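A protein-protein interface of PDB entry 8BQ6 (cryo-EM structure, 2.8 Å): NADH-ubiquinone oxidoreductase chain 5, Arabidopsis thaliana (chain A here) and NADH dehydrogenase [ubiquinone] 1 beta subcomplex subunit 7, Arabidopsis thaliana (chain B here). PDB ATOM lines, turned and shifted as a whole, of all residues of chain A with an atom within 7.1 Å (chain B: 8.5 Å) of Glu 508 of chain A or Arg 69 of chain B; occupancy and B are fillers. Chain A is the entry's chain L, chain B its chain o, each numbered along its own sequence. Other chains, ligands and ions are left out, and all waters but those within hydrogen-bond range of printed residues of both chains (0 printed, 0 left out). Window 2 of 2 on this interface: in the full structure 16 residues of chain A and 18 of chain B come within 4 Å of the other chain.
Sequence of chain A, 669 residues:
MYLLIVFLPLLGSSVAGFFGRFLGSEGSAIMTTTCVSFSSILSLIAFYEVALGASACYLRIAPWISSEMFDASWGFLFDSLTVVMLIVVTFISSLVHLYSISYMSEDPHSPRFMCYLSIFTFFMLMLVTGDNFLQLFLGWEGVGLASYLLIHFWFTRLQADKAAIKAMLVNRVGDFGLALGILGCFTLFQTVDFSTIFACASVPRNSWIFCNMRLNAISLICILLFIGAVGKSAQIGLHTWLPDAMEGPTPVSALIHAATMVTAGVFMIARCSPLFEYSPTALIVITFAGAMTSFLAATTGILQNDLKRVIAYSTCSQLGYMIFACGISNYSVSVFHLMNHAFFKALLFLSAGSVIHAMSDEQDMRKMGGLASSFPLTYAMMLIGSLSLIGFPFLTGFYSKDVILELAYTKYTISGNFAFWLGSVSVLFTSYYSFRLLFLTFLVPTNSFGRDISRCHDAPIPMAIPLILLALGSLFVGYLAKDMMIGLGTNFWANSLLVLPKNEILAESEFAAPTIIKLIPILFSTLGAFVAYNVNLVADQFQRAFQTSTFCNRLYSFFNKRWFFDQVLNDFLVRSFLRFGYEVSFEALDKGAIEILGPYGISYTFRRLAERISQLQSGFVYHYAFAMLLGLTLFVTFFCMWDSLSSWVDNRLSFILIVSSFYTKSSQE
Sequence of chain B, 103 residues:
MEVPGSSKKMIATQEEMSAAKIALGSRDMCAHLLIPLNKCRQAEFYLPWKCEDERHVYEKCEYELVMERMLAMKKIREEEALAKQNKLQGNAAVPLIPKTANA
The side-chain carboxylate of Glu 508 of chain A is in salt-bridge range of the guanidinium group of Arg 69 of chain B (3.2 Å).
The side-chain hydroxyl (OH) of Tyr 63 of chain B is in hydrogen-bond range of the side-chain sulfur (SD) of Met 67 of chain B.
Among the printed residues, pairs that only touch across the chains: Glu 504 of chain A with Gly 25 of chain B, Leu 488 of chain A with Glu 62 of chain B, Ala 512 of chain A with Met 70 of chain B, Glu 508 of chain A with Val 66 of chain B, Phe 511 of chain A with Tyr 63 of chain B and Ala 512 of chain A with Val 66 of chain B.
No residue of chain B comes within 4 Å of Ala 507 of chain A.
Glu 508 of chain A touches just these residues of chain B: Val 66 (3.8 Å) and Arg 69 (3.2 Å).
Printed residues of chain B within 4 Å of Phe 511 of chain A: Tyr 63.
Printed residues of chain A within 4 Å of Gly 25 of chain B: Glu 504.
Of the printed residues of chain A, Glu 62 of chain B touches Leu 488.
Printed residues of chain A within 4 Å of Val 66 of chain B: Glu 508 (3.8 Å) and Ala 512 (3.9 Å).
Printed residues of chain A within 4 Å of Met 70 of chain B: Ala 512 (3.8 Å).
The nearest residue of chain A that does not touch Arg 69 of chain B is Ala 507 of chain A (6.0 Å).
The nearest printed residue of chain B that does not touch Leu 488 of chain A is Asp 28 of chain B (6.5 Å).
Of the 18 printed residues of chain B, 6 touch a printed residue of chain A.
Hydrophobic or aromatic side chains of chain B that line the printed part of chain A: Tyr 63, Val 66 and Met 70.
Along chain B the printed residues that touch a printed residue of chain A span positions 25 to 70.
Printed residues of chain A that touch a printed residue of chain B: Leu 488, Glu 504, Glu 508, Phe 511 and Ala 512.
Among the printed residues, 7 pairs touch across the chains.
Among the printed residues, Asp or Glu carboxylates within 4 Å of a Lys or Arg side-chain nitrogen of the other chain: Glu 508 of chain A with Arg 69 of chain B.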
ATOM      1  N   GLU A 406      -1.227 -17.643  16.485  1.00  0.00           N
ATOM      2  CA  GLU A 406      -0.144 -18.449  15.934  1.00  0.00           C
ATOM      3  C   GLU A 406       0.138 -18.083  14.484  1.00  0.00           C
ATOM      4  O   GLU A 406       1.299 -17.947  14.084  1.00  0.00           O
ATOM      5  CB  GLU A 406      -0.495 -19.928  16.054  1.00  0.00           C
ATOM      6  CG  GLU A 406      -0.136 -20.528  17.386  1.00  0.00           C
ATOM      7  CD  GLU A 406      -1.068 -21.650  17.772  1.00  0.00           C
ATOM      8  OE1 GLU A 406      -1.438 -22.449  16.886  1.00  0.00           O
ATOM      9  OE2 GLU A 406      -1.421 -21.738  18.965  1.00  0.00           O
ATOM     10  N   LEU A 407      -0.918 -17.914  13.684  1.00  0.00           N
ATOM     11  CA  LEU A 407      -0.752 -17.580  12.272  1.00  0.00           C
ATOM     12  C   LEU A 407      -0.129 -16.202  12.091  1.00  0.00           C
ATOM     13  O   LEU A 407       0.613 -15.973  11.127  1.00  0.00           O
ATOM     14  CB  LEU A 407      -2.100 -17.644  11.560  1.00  0.00           C
ATOM     15  CG  LEU A 407      -2.648 -19.027  11.225  1.00  0.00           C
ATOM     16  CD1 LEU A 407      -4.150 -18.972  11.037  1.00  0.00           C
ATOM     17  CD2 LEU A 407      -1.975 -19.527   9.972  1.00  0.00           C
ATOM     18  N   TYR A 409       2.060 -14.774  14.082  1.00  0.00           N
ATOM     19  CA  TYR A 409       3.488 -14.953  14.299  1.00  0.00           C
ATOM     20  C   TYR A 409       4.150 -15.556  13.068  1.00  0.00           C
ATOM     21  O   TYR A 409       5.269 -15.179  12.705  1.00  0.00           O
ATOM     22  CB  TYR A 409       3.715 -15.834  15.524  1.00  0.00           C
ATOM     23  CG  TYR A 409       5.150 -16.228  15.737  1.00  0.00           C
ATOM     24  CD1 TYR A 409       6.018 -15.377  16.398  1.00  0.00           C
ATOM     25  CD2 TYR A 409       5.631 -17.457  15.305  1.00  0.00           C
ATOM     26  CE1 TYR A 409       7.322 -15.719  16.604  1.00  0.00           C
ATOM     27  CE2 TYR A 409       6.947 -17.812  15.511  1.00  0.00           C
ATOM     28  CZ  TYR A 409       7.784 -16.936  16.163  1.00  0.00           C
ATOM     29  OH  TYR A 409       9.096 -17.266  16.382  1.00  0.00           O
ATOM     30  N   THR A 410       3.470 -16.493  12.416  1.00  0.00           N
ATOM     31  CA  THR A 410       4.014 -17.152  11.239  1.00  0.00           C
ATOM     32  C   THR A 410       4.061 -16.246  10.017  1.00  0.00           C
ATOM     33  O   THR A 410       4.862 -16.496   9.111  1.00  0.00           O
ATOM     34  CB  THR A 410       3.195 -18.406  10.935  1.00  0.00           C
ATOM     35  OG1 THR A 410       2.870 -19.059  12.167  1.00  0.00           O
ATOM     36  CG2 THR A 410       3.991 -19.362  10.069  1.00  0.00           C
ATOM     37  N   LEU A 488      -6.248 -29.369   8.761  1.00  0.00           N
ATOM     38  CA  LEU A 488      -5.219 -29.198   7.745  1.00  0.00           C
ATOM     39  C   LEU A 488      -5.606 -29.938   6.471  1.00  0.00           C
ATOM     40  O   LEU A 488      -5.836 -31.150   6.487  1.00  0.00           O
ATOM     41  CB  LEU A 488      -3.880 -29.696   8.293  1.00  0.00           C
ATOM     42  CG  LEU A 488      -2.599 -29.193   7.627  1.00  0.00           C
ATOM     43  CD1 LEU A 488      -1.424 -29.197   8.600  1.00  0.00           C
ATOM     44  CD2 LEU A 488      -2.276 -30.034   6.423  1.00  0.00           C
ATOM     45  N   LYS A 502       0.778 -19.347  -2.553  1.00  0.00           N
ATOM     46  CA  LYS A 502       1.874 -18.562  -1.992  1.00  0.00           C
ATOM     47  C   LYS A 502       1.555 -18.009  -0.611  1.00  0.00           C
ATOM     48  O   LYS A 502       2.472 -17.592   0.106  1.00  0.00           O
ATOM     49  CB  LYS A 502       2.225 -17.407  -2.927  1.00  0.00           C
ATOM     50  CG  LYS A 502       1.163 -16.332  -2.991  1.00  0.00           C
ATOM     51  CD  LYS A 502       1.111 -15.712  -4.370  1.00  0.00           C
ATOM     52  CE  LYS A 502       0.145 -14.548  -4.412  1.00  0.00           C
ATOM     53  NZ  LYS A 502       0.674 -13.348  -3.712  1.00  0.00           N
ATOM     54  N   ASN A 503       0.284 -17.986  -0.223  1.00  0.00           N
ATOM     55  CA  ASN A 503      -0.144 -17.394   1.034  1.00  0.00           C
ATOM     56  C   ASN A 503      -0.460 -18.429   2.105  1.00  0.00           C
ATOM     57  O   ASN A 503      -0.911 -18.057   3.192  1.00  0.00           O
ATOM     58  CB  ASN A 503      -1.370 -16.511   0.789  1.00  0.00           C
ATOM     59  CG  ASN A 503      -1.023 -15.213   0.084  1.00  0.00           C
ATOM     60  OD1 ASN A 503       0.029 -14.622   0.322  1.00  0.00           O
ATOM     61  ND2 ASN A 503      -1.892 -14.788  -0.821  1.00  0.00           N
ATOM     62  N   GLU A 504      -0.234 -19.712   1.836  1.00  0.00           N
ATOM     63  CA  GLU A 504      -0.617 -20.748   2.787  1.00  0.00           C
ATOM     64  C   GLU A 504       0.435 -20.878   3.881  1.00  0.00           C
ATOM     65  O   GLU A 504       1.623 -21.060   3.594  1.00  0.00           O
ATOM     66  CB  GLU A 504      -0.823 -22.075   2.066  1.00  0.00           C
ATOM     67  CG  GLU A 504      -1.783 -21.970   0.903  1.00  0.00           C
ATOM     68  CD  GLU A 504      -3.216 -22.252   1.311  1.00  0.00           C
ATOM     69  OE1 GLU A 504      -3.494 -22.294   2.527  1.00  0.00           O
ATOM     70  OE2 GLU A 504      -4.070 -22.415   0.416  1.00  0.00           O
ATOM     71  N   ILE A 505      -0.005 -20.765   5.136  1.00  0.00           N
ATOM     72  CA  ILE A 505       0.892 -20.763   6.282  1.00  0.00           C
ATOM     73  C   ILE A 505       0.419 -21.669   7.409  1.00  0.00           C
ATOM     74  O   ILE A 505       1.066 -21.714   8.457  1.00  0.00           O
ATOM     75  CB  ILE A 505       1.108 -19.332   6.817  1.00  0.00           C
ATOM     76  CG1 ILE A 505      -0.226 -18.604   6.957  1.00  0.00           C
ATOM     77  CG2 ILE A 505       2.004 -18.534   5.894  1.00  0.00           C
ATOM     78  CD1 ILE A 505      -0.116 -17.298   7.701  1.00  0.00           C
ATOM     79  N   LEU A 506      -0.693 -22.391   7.241  1.00  0.00           N
ATOM     80  CA  LEU A 506      -1.256 -23.142   8.363  1.00  0.00           C
ATOM     81  C   LEU A 506      -0.302 -24.229   8.844  1.00  0.00           C
ATOM     82  O   LEU A 506      -0.109 -24.407  10.052  1.00  0.00           O
ATOM     83  CB  LEU A 506      -2.608 -23.750   7.988  1.00  0.00           C
ATOM     84  CG  LEU A 506      -3.272 -24.517   9.142  1.00  0.00           C
ATOM     85  CD1 LEU A 506      -3.792 -23.575  10.222  1.00  0.00           C
ATOM     86  CD2 LEU A 506      -4.383 -25.437   8.654  1.00  0.00           C
ATOM     87  N   ALA A 507       0.302 -24.969   7.913  1.00  0.00           N
ATOM     88  CA  ALA A 507       1.201 -26.051   8.304  1.00  0.00           C
ATOM     89  C   ALA A 507       2.400 -25.516   9.081  1.00  0.00           C
ATOM     90  O   ALA A 507       2.736 -26.030  10.154  1.00  0.00           O
ATOM     91  CB  ALA A 507       1.653 -26.826   7.068  1.00  0.00           C
ATOM     92  N   GLU A 508       3.030 -24.467   8.558  1.00  0.00           N
ATOM     93  CA  GLU A 508       4.191 -23.850   9.256  1.00  0.00           C
ATOM     94  C   GLU A 508       3.747 -23.277  10.609  1.00  0.00           C
ATOM     95  O   GLU A 508       4.572 -23.265  11.534  1.00  0.00           O
ATOM     96  CB  GLU A 508       4.825 -22.775   8.375  1.00  0.00           C
ATOM     97  CG  GLU A 508       5.230 -23.271   7.002  1.00  0.00           C
ATOM     98  CD  GLU A 508       4.282 -22.894   5.877  1.00  0.00           C
ATOM     99  OE1 GLU A 508       3.190 -23.483   5.809  1.00  0.00           O
ATOM    100  OE2 GLU A 508       4.640 -22.020   5.071  1.00  0.00           O
ATOM    101  N   SER A 509       2.496 -22.819  10.720  1.00  0.00           N
ATOM    102  CA  SER A 509       2.033 -22.222  11.969  1.00  0.00           C
ATOM    103  C   SER A 509       1.843 -23.278  13.049  1.00  0.00           C
ATOM    104  O   SER A 509       1.884 -22.967  14.246  1.00  0.00           O
ATOM    105  CB  SER A 509       0.733 -21.458  11.726  1.00  0.00           C
ATOM    106  OG  SER A 509      -0.393 -22.251  12.058  1.00  0.00           O
ATOM    107  N   GLU A 510       1.640 -24.529  12.650  1.00  0.00           N
ATOM    108  CA  GLU A 510       1.388 -25.595  13.607  1.00  0.00           C
ATOM    109  C   GLU A 510       2.635 -26.415  13.926  1.00  0.00           C
ATOM    110  O   GLU A 510       2.685 -27.047  14.986  1.00  0.00           O
ATOM    111  CB  GLU A 510       0.261 -26.490  13.074  1.00  0.00           C
ATOM    112  CG  GLU A 510      -0.074 -27.750  13.878  1.00  0.00           C
ATOM    113  CD  GLU A 510      -0.700 -27.470  15.238  1.00  0.00           C
ATOM    114  OE1 GLU A 510      -1.691 -28.147  15.582  1.00  0.00           O
ATOM    115  OE2 GLU A 510      -0.192 -26.608  15.982  1.00  0.00           O
ATOM    116  N   PHE A 511       3.660 -26.380  13.073  1.00  0.00           N
ATOM    117  CA  PHE A 511       4.802 -27.270  13.244  1.00  0.00           C
ATOM    118  C   PHE A 511       6.117 -26.524  13.446  1.00  0.00           C
ATOM    119  O   PHE A 511       6.937 -26.928  14.276  1.00  0.00           O
ATOM    120  CB  PHE A 511       4.893 -28.207  12.040  1.00  0.00           C
ATOM    121  CG  PHE A 511       3.709 -29.117  11.903  1.00  0.00           C
ATOM    122  CD1 PHE A 511       3.171 -29.745  13.013  1.00  0.00           C
ATOM    123  CD2 PHE A 511       3.110 -29.313  10.672  1.00  0.00           C
ATOM    124  CE1 PHE A 511       2.077 -30.573  12.892  1.00  0.00           C
ATOM    125  CE2 PHE A 511       2.013 -30.135  10.545  1.00  0.00           C
ATOM    126  CZ  PHE A 511       1.494 -30.765  11.655  1.00  0.00           C
ATOM    127  N   ALA A 512       6.335 -25.433  12.713  1.00  0.00           N
ATOM    128  CA  ALA A 512       7.606 -24.719  12.757  1.00  0.00           C
ATOM    129  C   ALA A 512       7.670 -23.681  13.871  1.00  0.00           C
ATOM    130  O   ALA A 512       8.665 -22.955  13.970  1.00  0.00           O
ATOM    131  CB  ALA A 512       7.885 -24.050  11.410  1.00  0.00           C
ATOM    132  N   ALA A 513       6.637 -23.587  14.701  1.00  0.00           N
ATOM    133  CA  ALA A 513       6.611 -22.576  15.750  1.00  0.00           C
ATOM    134  C   ALA A 513       7.239 -23.108  17.035  1.00  0.00           C
ATOM    135  O   ALA A 513       6.979 -24.249  17.426  1.00  0.00           O
ATOM    136  CB  ALA A 513       5.184 -22.133  16.037  1.00  0.00           C
ATOM    137  N   LYS A 518       3.047 -20.781  21.479  1.00  0.00           N
ATOM    138  CA  LYS A 518       1.703 -21.292  21.704  1.00  0.00           C
ATOM    139  C   LYS A 518       1.268 -21.190  23.160  1.00  0.00           C
ATOM    140  O   LYS A 518       0.093 -21.426  23.457  1.00  0.00           O
ATOM    141  CB  LYS A 518       1.625 -22.743  21.243  1.00  0.00           C
ATOM    142  CG  LYS A 518       2.220 -22.955  19.869  1.00  0.00           C
ATOM    143  CD  LYS A 518       2.892 -24.309  19.779  1.00  0.00           C
ATOM    144  CE  LYS A 518       2.530 -25.008  18.487  1.00  0.00           C
ATOM    145  NZ  LYS A 518       3.228 -24.398  17.327  1.00  0.00           N
ATOM    146  N   LYS B   8      11.511 -37.343  -1.180  1.00  0.00           N
ATOM    147  CA  LYS B   8      10.103 -36.992  -1.331  1.00  0.00           C
ATOM    148  C   LYS B   8       9.814 -36.602  -2.773  1.00  0.00           C
ATOM    149  O   LYS B   8      10.284 -35.566  -3.243  1.00  0.00           O
ATOM    150  CB  LYS B   8       9.735 -35.849  -0.386  1.00  0.00           C
ATOM    151  CG  LYS B   8       9.936 -36.186   1.077  1.00  0.00           C
ATOM    152  CD  LYS B   8       9.612 -35.008   1.972  1.00  0.00           C
ATOM    153  CE  LYS B   8       9.889 -35.351   3.421  1.00  0.00           C
ATOM    154  NZ  LYS B   8       9.045 -36.502   3.837  1.00  0.00           N
ATOM    155  N   GLY B  25      -4.012 -24.822  -2.545  1.00  0.00           N
ATOM    156  CA  GLY B  25      -2.969 -24.685  -1.551  1.00  0.00           C
ATOM    157  C   GLY B  25      -2.574 -25.979  -0.871  1.00  0.00           C
ATOM    158  O   GLY B  25      -1.540 -26.005  -0.196  1.00  0.00           O
ATOM    159  N   ASP B  28       0.257 -30.235  -2.626  1.00  0.00           N
ATOM    160  CA  ASP B  28       1.688 -30.349  -2.396  1.00  0.00           C
ATOM    161  C   ASP B  28       2.097 -31.826  -2.394  1.00  0.00           C
ATOM    162  O   ASP B  28       1.313 -32.702  -2.776  1.00  0.00           O
ATOM    163  CB  ASP B  28       2.066 -29.617  -1.102  1.00  0.00           C
ATOM    164  CG  ASP B  28       1.211 -30.025   0.077  1.00  0.00           C
ATOM    165  OD1 ASP B  28       0.264 -30.815  -0.112  1.00  0.00           O
ATOM    166  OD2 ASP B  28       1.485 -29.548   1.196  1.00  0.00           O
ATOM    167  N   GLU B  62       3.143 -33.726   6.312  1.00  0.00           N
ATOM    168  CA  GLU B  62       3.226 -32.270   6.253  1.00  0.00           C
ATOM    169  C   GLU B  62       4.254 -31.736   7.240  1.00  0.00           C
ATOM    170  O   GLU B  62       4.919 -30.731   6.969  1.00  0.00           O
ATOM    171  CB  GLU B  62       1.856 -31.646   6.510  1.00  0.00           C
ATOM    172  CG  GLU B  62       0.845 -31.914   5.415  1.00  0.00           C
ATOM    173  CD  GLU B  62       1.040 -31.027   4.199  1.00  0.00           C
ATOM    174  OE1 GLU B  62       1.961 -30.185   4.203  1.00  0.00           O
ATOM    175  OE2 GLU B  62       0.273 -31.178   3.229  1.00  0.00           O
ATOM    176  N   TYR B  63       4.388 -32.387   8.398  1.00  0.00           N
ATOM    177  CA  TYR B  63       5.473 -32.052   9.316  1.00  0.00           C
ATOM    178  C   TYR B  63       6.825 -32.310   8.675  1.00  0.00           C
ATOM    179  O   TYR B  63       7.764 -31.520   8.838  1.00  0.00           O
ATOM    180  CB  TYR B  63       5.346 -32.868  10.601  1.00  0.00           C
ATOM    181  CG  TYR B  63       6.521 -32.737  11.550  1.00  0.00           C
ATOM    182  CD1 TYR B  63       7.561 -33.660  11.533  1.00  0.00           C
ATOM    183  CD2 TYR B  63       6.569 -31.720  12.489  1.00  0.00           C
ATOM    184  CE1 TYR B  63       8.628 -33.550  12.403  1.00  0.00           C
ATOM    185  CE2 TYR B  63       7.626 -31.608  13.365  1.00  0.00           C
ATOM    186  CZ  TYR B  63       8.653 -32.522  13.319  1.00  0.00           C
ATOM    187  OH  TYR B  63       9.708 -32.404  14.195  1.00  0.00           O
ATOM    188  N   GLU B  64       6.947 -33.424   7.954  1.00  0.00           N
ATOM    189  CA  GLU B  64       8.202 -33.749   7.288  1.00  0.00           C
ATOM    190  C   GLU B  64       8.559 -32.693   6.250  1.00  0.00           C
ATOM    191  O   GLU B  64       9.731 -32.340   6.092  1.00  0.00           O
ATOM    192  CB  GLU B  64       8.096 -35.130   6.646  1.00  0.00           C
ATOM    193  CG  GLU B  64       8.611 -36.260   7.522  1.00  0.00           C
ATOM    194  CD  GLU B  64       9.297 -37.343   6.721  1.00  0.00           C
ATOM    195  OE1 GLU B  64       8.601 -38.275   6.267  1.00  0.00           O
ATOM    196  OE2 GLU B  64      10.530 -37.259   6.536  1.00  0.00           O
ATOM    197  N   LEU B  65       7.558 -32.172   5.535  1.00  0.00           N
ATOM    198  CA  LEU B  65       7.837 -31.188   4.495  1.00  0.00           C
ATOM    199  C   LEU B  65       8.356 -29.886   5.092  1.00  0.00           C
ATOM    200  O   LEU B  65       9.325 -29.305   4.591  1.00  0.00           O
ATOM    201  CB  LEU B  65       6.582 -30.935   3.660  1.00  0.00           C
ATOM    202  CG  LEU B  65       6.551 -31.571   2.269  1.00  0.00           C
ATOM    203  CD1 LEU B  65       7.666 -31.046   1.382  1.00  0.00           C
ATOM    204  CD2 LEU B  65       6.631 -33.078   2.394  1.00  0.00           C
ATOM    205  N   VAL B  66       7.724 -29.413   6.168  1.00  0.00           N
ATOM    206  CA  VAL B  66       8.099 -28.121   6.741  1.00  0.00           C
ATOM    207  C   VAL B  66       9.481 -28.199   7.373  1.00  0.00           C
ATOM    208  O   VAL B  66      10.263 -27.241   7.315  1.00  0.00           O
ATOM    209  CB  VAL B  66       7.039 -27.651   7.752  1.00  0.00           C
ATOM    210  CG1 VAL B  66       7.347 -26.240   8.223  1.00  0.00           C
ATOM    211  CG2 VAL B  66       5.656 -27.707   7.133  1.00  0.00           C
ATOM    212  N   MET B  67       9.788 -29.339   7.992  1.00  0.00           N
ATOM    213  CA  MET B  67      11.144 -29.531   8.571  1.00  0.00           C
ATOM    214  C   MET B  67      12.179 -29.470   7.445  1.00  0.00           C
ATOM    215  O   MET B  67      13.229 -28.854   7.653  1.00  0.00           O
ATOM    216  CB  MET B  67      11.238 -30.882   9.283  1.00  0.00           C
ATOM    217  CG  MET B  67      10.316 -30.991  10.477  1.00  0.00           C
ATOM    218  SD  MET B  67      10.715 -29.800  11.780  1.00  0.00           S
ATOM    219  CE  MET B  67       9.428 -28.582  11.523  1.00  0.00           C
ATOM    220  N   GLU B  68      11.883 -30.085   6.302  1.00  0.00           N
ATOM    221  CA  GLU B  68      12.825 -30.110   5.154  1.00  0.00           C
ATOM    222  C   GLU B  68      13.166 -28.680   4.716  1.00  0.00           C
ATOM    223  O   GLU B  68      14.367 -28.392   4.569  1.00  0.00           O
ATOM    224  CB  GLU B  68      12.193 -30.918   4.025  1.00  0.00           C
ATOM    225  CG  GLU B  68      13.189 -31.531   3.060  1.00  0.00           C
ATOM    226  CD  GLU B  68      12.581 -31.954   1.732  1.00  0.00           C
ATOM    227  OE1 GLU B  68      11.352 -32.152   1.678  1.00  0.00           O
ATOM    228  OE2 GLU B  68      13.337 -32.082   0.752  1.00  0.00           O
ATOM    229  N   ARG B  69      12.154 -27.820   4.532  1.00  0.00           N
ATOM    230  CA  ARG B  69      12.375 -26.403   4.131  1.00  0.00           C
ATOM    231  C   ARG B  69      13.031 -25.628   5.275  1.00  0.00           C
ATOM    232  O   ARG B  69      13.837 -24.728   4.976  1.00  0.00           O
ATOM    233  CB  ARG B  69      11.056 -25.740   3.739  1.00  0.00           C
ATOM    234  CG  ARG B  69      10.366 -26.375   2.541  1.00  0.00           C
ATOM    235  CD  ARG B  69       8.885 -26.056   2.510  1.00  0.00           C
ATOM    236  NE  ARG B  69       8.610 -24.715   3.008  1.00  0.00           N
ATOM    237  CZ  ARG B  69       7.608 -24.398   3.817  1.00  0.00           C
ATOM    238  NH1 ARG B  69       6.759 -25.326   4.223  1.00  0.00           N
ATOM    239  NH2 ARG B  69       7.456 -23.148   4.210  1.00  0.00           N
ATOM    240  N   MET B  70      12.699 -25.953   6.525  1.00  0.00           N
ATOM    241  CA  MET B  70      13.361 -25.310   7.689  1.00  0.00           C
ATOM    242  C   MET B  70      14.862 -25.621   7.654  1.00  0.00           C
ATOM    243  O   MET B  70      15.647 -24.692   7.909  1.00  0.00           O
ATOM    244  CB  MET B  70      12.780 -25.833   9.005  1.00  0.00           C
ATOM    245  CG  MET B  70      11.650 -24.996   9.559  1.00  0.00           C
ATOM    246  SD  MET B  70      11.487 -25.204  11.347  1.00  0.00           S
ATOM    247  CE  MET B  70      12.583 -23.914  11.935  1.00  0.00           C
ATOM    248  N   LEU B  71      15.237 -26.869   7.345  1.00  0.00           N
ATOM    249  CA  LEU B  71      16.666 -27.290   7.310  1.00  0.00           C
ATOM    250  C   LEU B  71      17.374 -26.645   6.118  1.00  0.00           C
ATOM    251  O   LEU B  71      18.571 -26.344   6.245  1.00  0.00           O
ATOM    252  CB  LEU B  71      16.732 -28.817   7.207  1.00  0.00           C
ATOM    253  CG  LEU B  71      16.702 -29.554   8.542  1.00  0.00           C
ATOM    254  CD1 LEU B  71      16.101 -30.941   8.385  1.00  0.00           C
ATOM    255  CD2 LEU B  71      18.098 -29.641   9.140  1.00  0.00           C
ATOM    256  N   ALA B  72      16.667 -26.464   5.001  1.00  0.00           N
ATOM    257  CA  ALA B  72      17.261 -25.809   3.814  1.00  0.00           C
ATOM    258  C   ALA B  72      17.638 -24.368   4.157  1.00  0.00           C
ATOM    259  O   ALA B  72      18.689 -23.911   3.693  1.00  0.00           O
ATOM    260  CB  ALA B  72      16.286 -25.864   2.671  1.00  0.00           C
ATOM    261  N   MET B  73      16.791 -23.674   4.924  1.00  0.00           N
ATOM    262  CA  MET B  73      17.108 -22.291   5.360  1.00  0.00           C
ATOM    263  C   MET B  73      18.199 -22.363   6.425  1.00  0.00           C
ATOM    264  O   MET B  73      19.113 -21.535   6.357  1.00  0.00           O
ATOM    265  CB  MET B  73      15.879 -21.604   5.950  1.00  0.00           C
ATOM    266  CG  MET B  73      16.123 -20.162   6.347  1.00  0.00           C
ATOM    267  SD  MET B  73      16.463 -19.102   4.925  1.00  0.00           S
ATOM    268  CE  MET B  73      14.825 -18.934   4.223  1.00  0.00           C
ATOM    269  N   LYS B  74      18.107 -23.313   7.364  1.00  0.00           N
ATOM    270  CA  LYS B  74      19.178 -23.494   8.380  1.00  0.00           C
ATOM    271  C   LYS B  74      20.517 -23.481   7.650  1.00  0.00           C
ATOM    272  O   LYS B  74      21.433 -22.794   8.135  1.00  0.00           O
ATOM    273  CB  LYS B  74      19.018 -24.820   9.125  1.00  0.00           C
ATOM    274  CG  LYS B  74      17.792 -24.931  10.017  1.00  0.00           C
ATOM    275  CD  LYS B  74      17.691 -26.276  10.699  1.00  0.00           C
ATOM    276  CE  LYS B  74      16.487 -26.389  11.609  1.00  0.00           C
ATOM    277  NZ  LYS B  74      16.402 -27.724  12.244  1.00  0.00           N
ATOM    278  N   LYS B  75      20.606 -24.188   6.520  1.00  0.00           N
ATOM    279  CA  LYS B  75      21.843 -24.138   5.708  1.00  0.00           C
ATOM    280  C   LYS B  75      22.052 -22.710   5.221  1.00  0.00           C
ATOM    281  O   LYS B  75      22.948 -22.117   5.704  1.00  0.00           O
ATOM    282  CB  LYS B  75      21.762 -25.105   4.525  1.00  0.00           C
ATOM    283  CG  LYS B  75      22.420 -26.457   4.749  1.00  0.00           C
ATOM    284  CD  LYS B  75      22.727 -27.186   3.460  1.00  0.00           C
ATOM    285  CE  LYS B  75      23.925 -26.620   2.729  1.00  0.00           C
ATOM    286  NZ  LYS B  75      25.191 -26.871   3.457  1.00  0.00           N
ATOM    287  N   ILE B  76      21.177 -22.147   4.404  1.00  0.00           N
ATOM    288  CA  ILE B  76      21.364 -20.848   3.754  1.00  0.00           C
ATOM    289  C   ILE B  76      21.801 -19.796   4.766  1.00  0.00           C
ATOM    290  O   ILE B  76      22.638 -18.932   4.475  1.00  0.00           O
ATOM    291  CB  ILE B  76      20.070 -20.439   3.033  1.00  0.00           C
ATOM    292  CG1 ILE B  76      19.953 -21.203   1.715  1.00  0.00           C
ATOM    293  CG2 ILE B  76      20.020 -18.936   2.804  1.00  0.00           C
ATOM    294  CD1 ILE B  76      18.538 -21.361   1.231  1.00  0.00           C
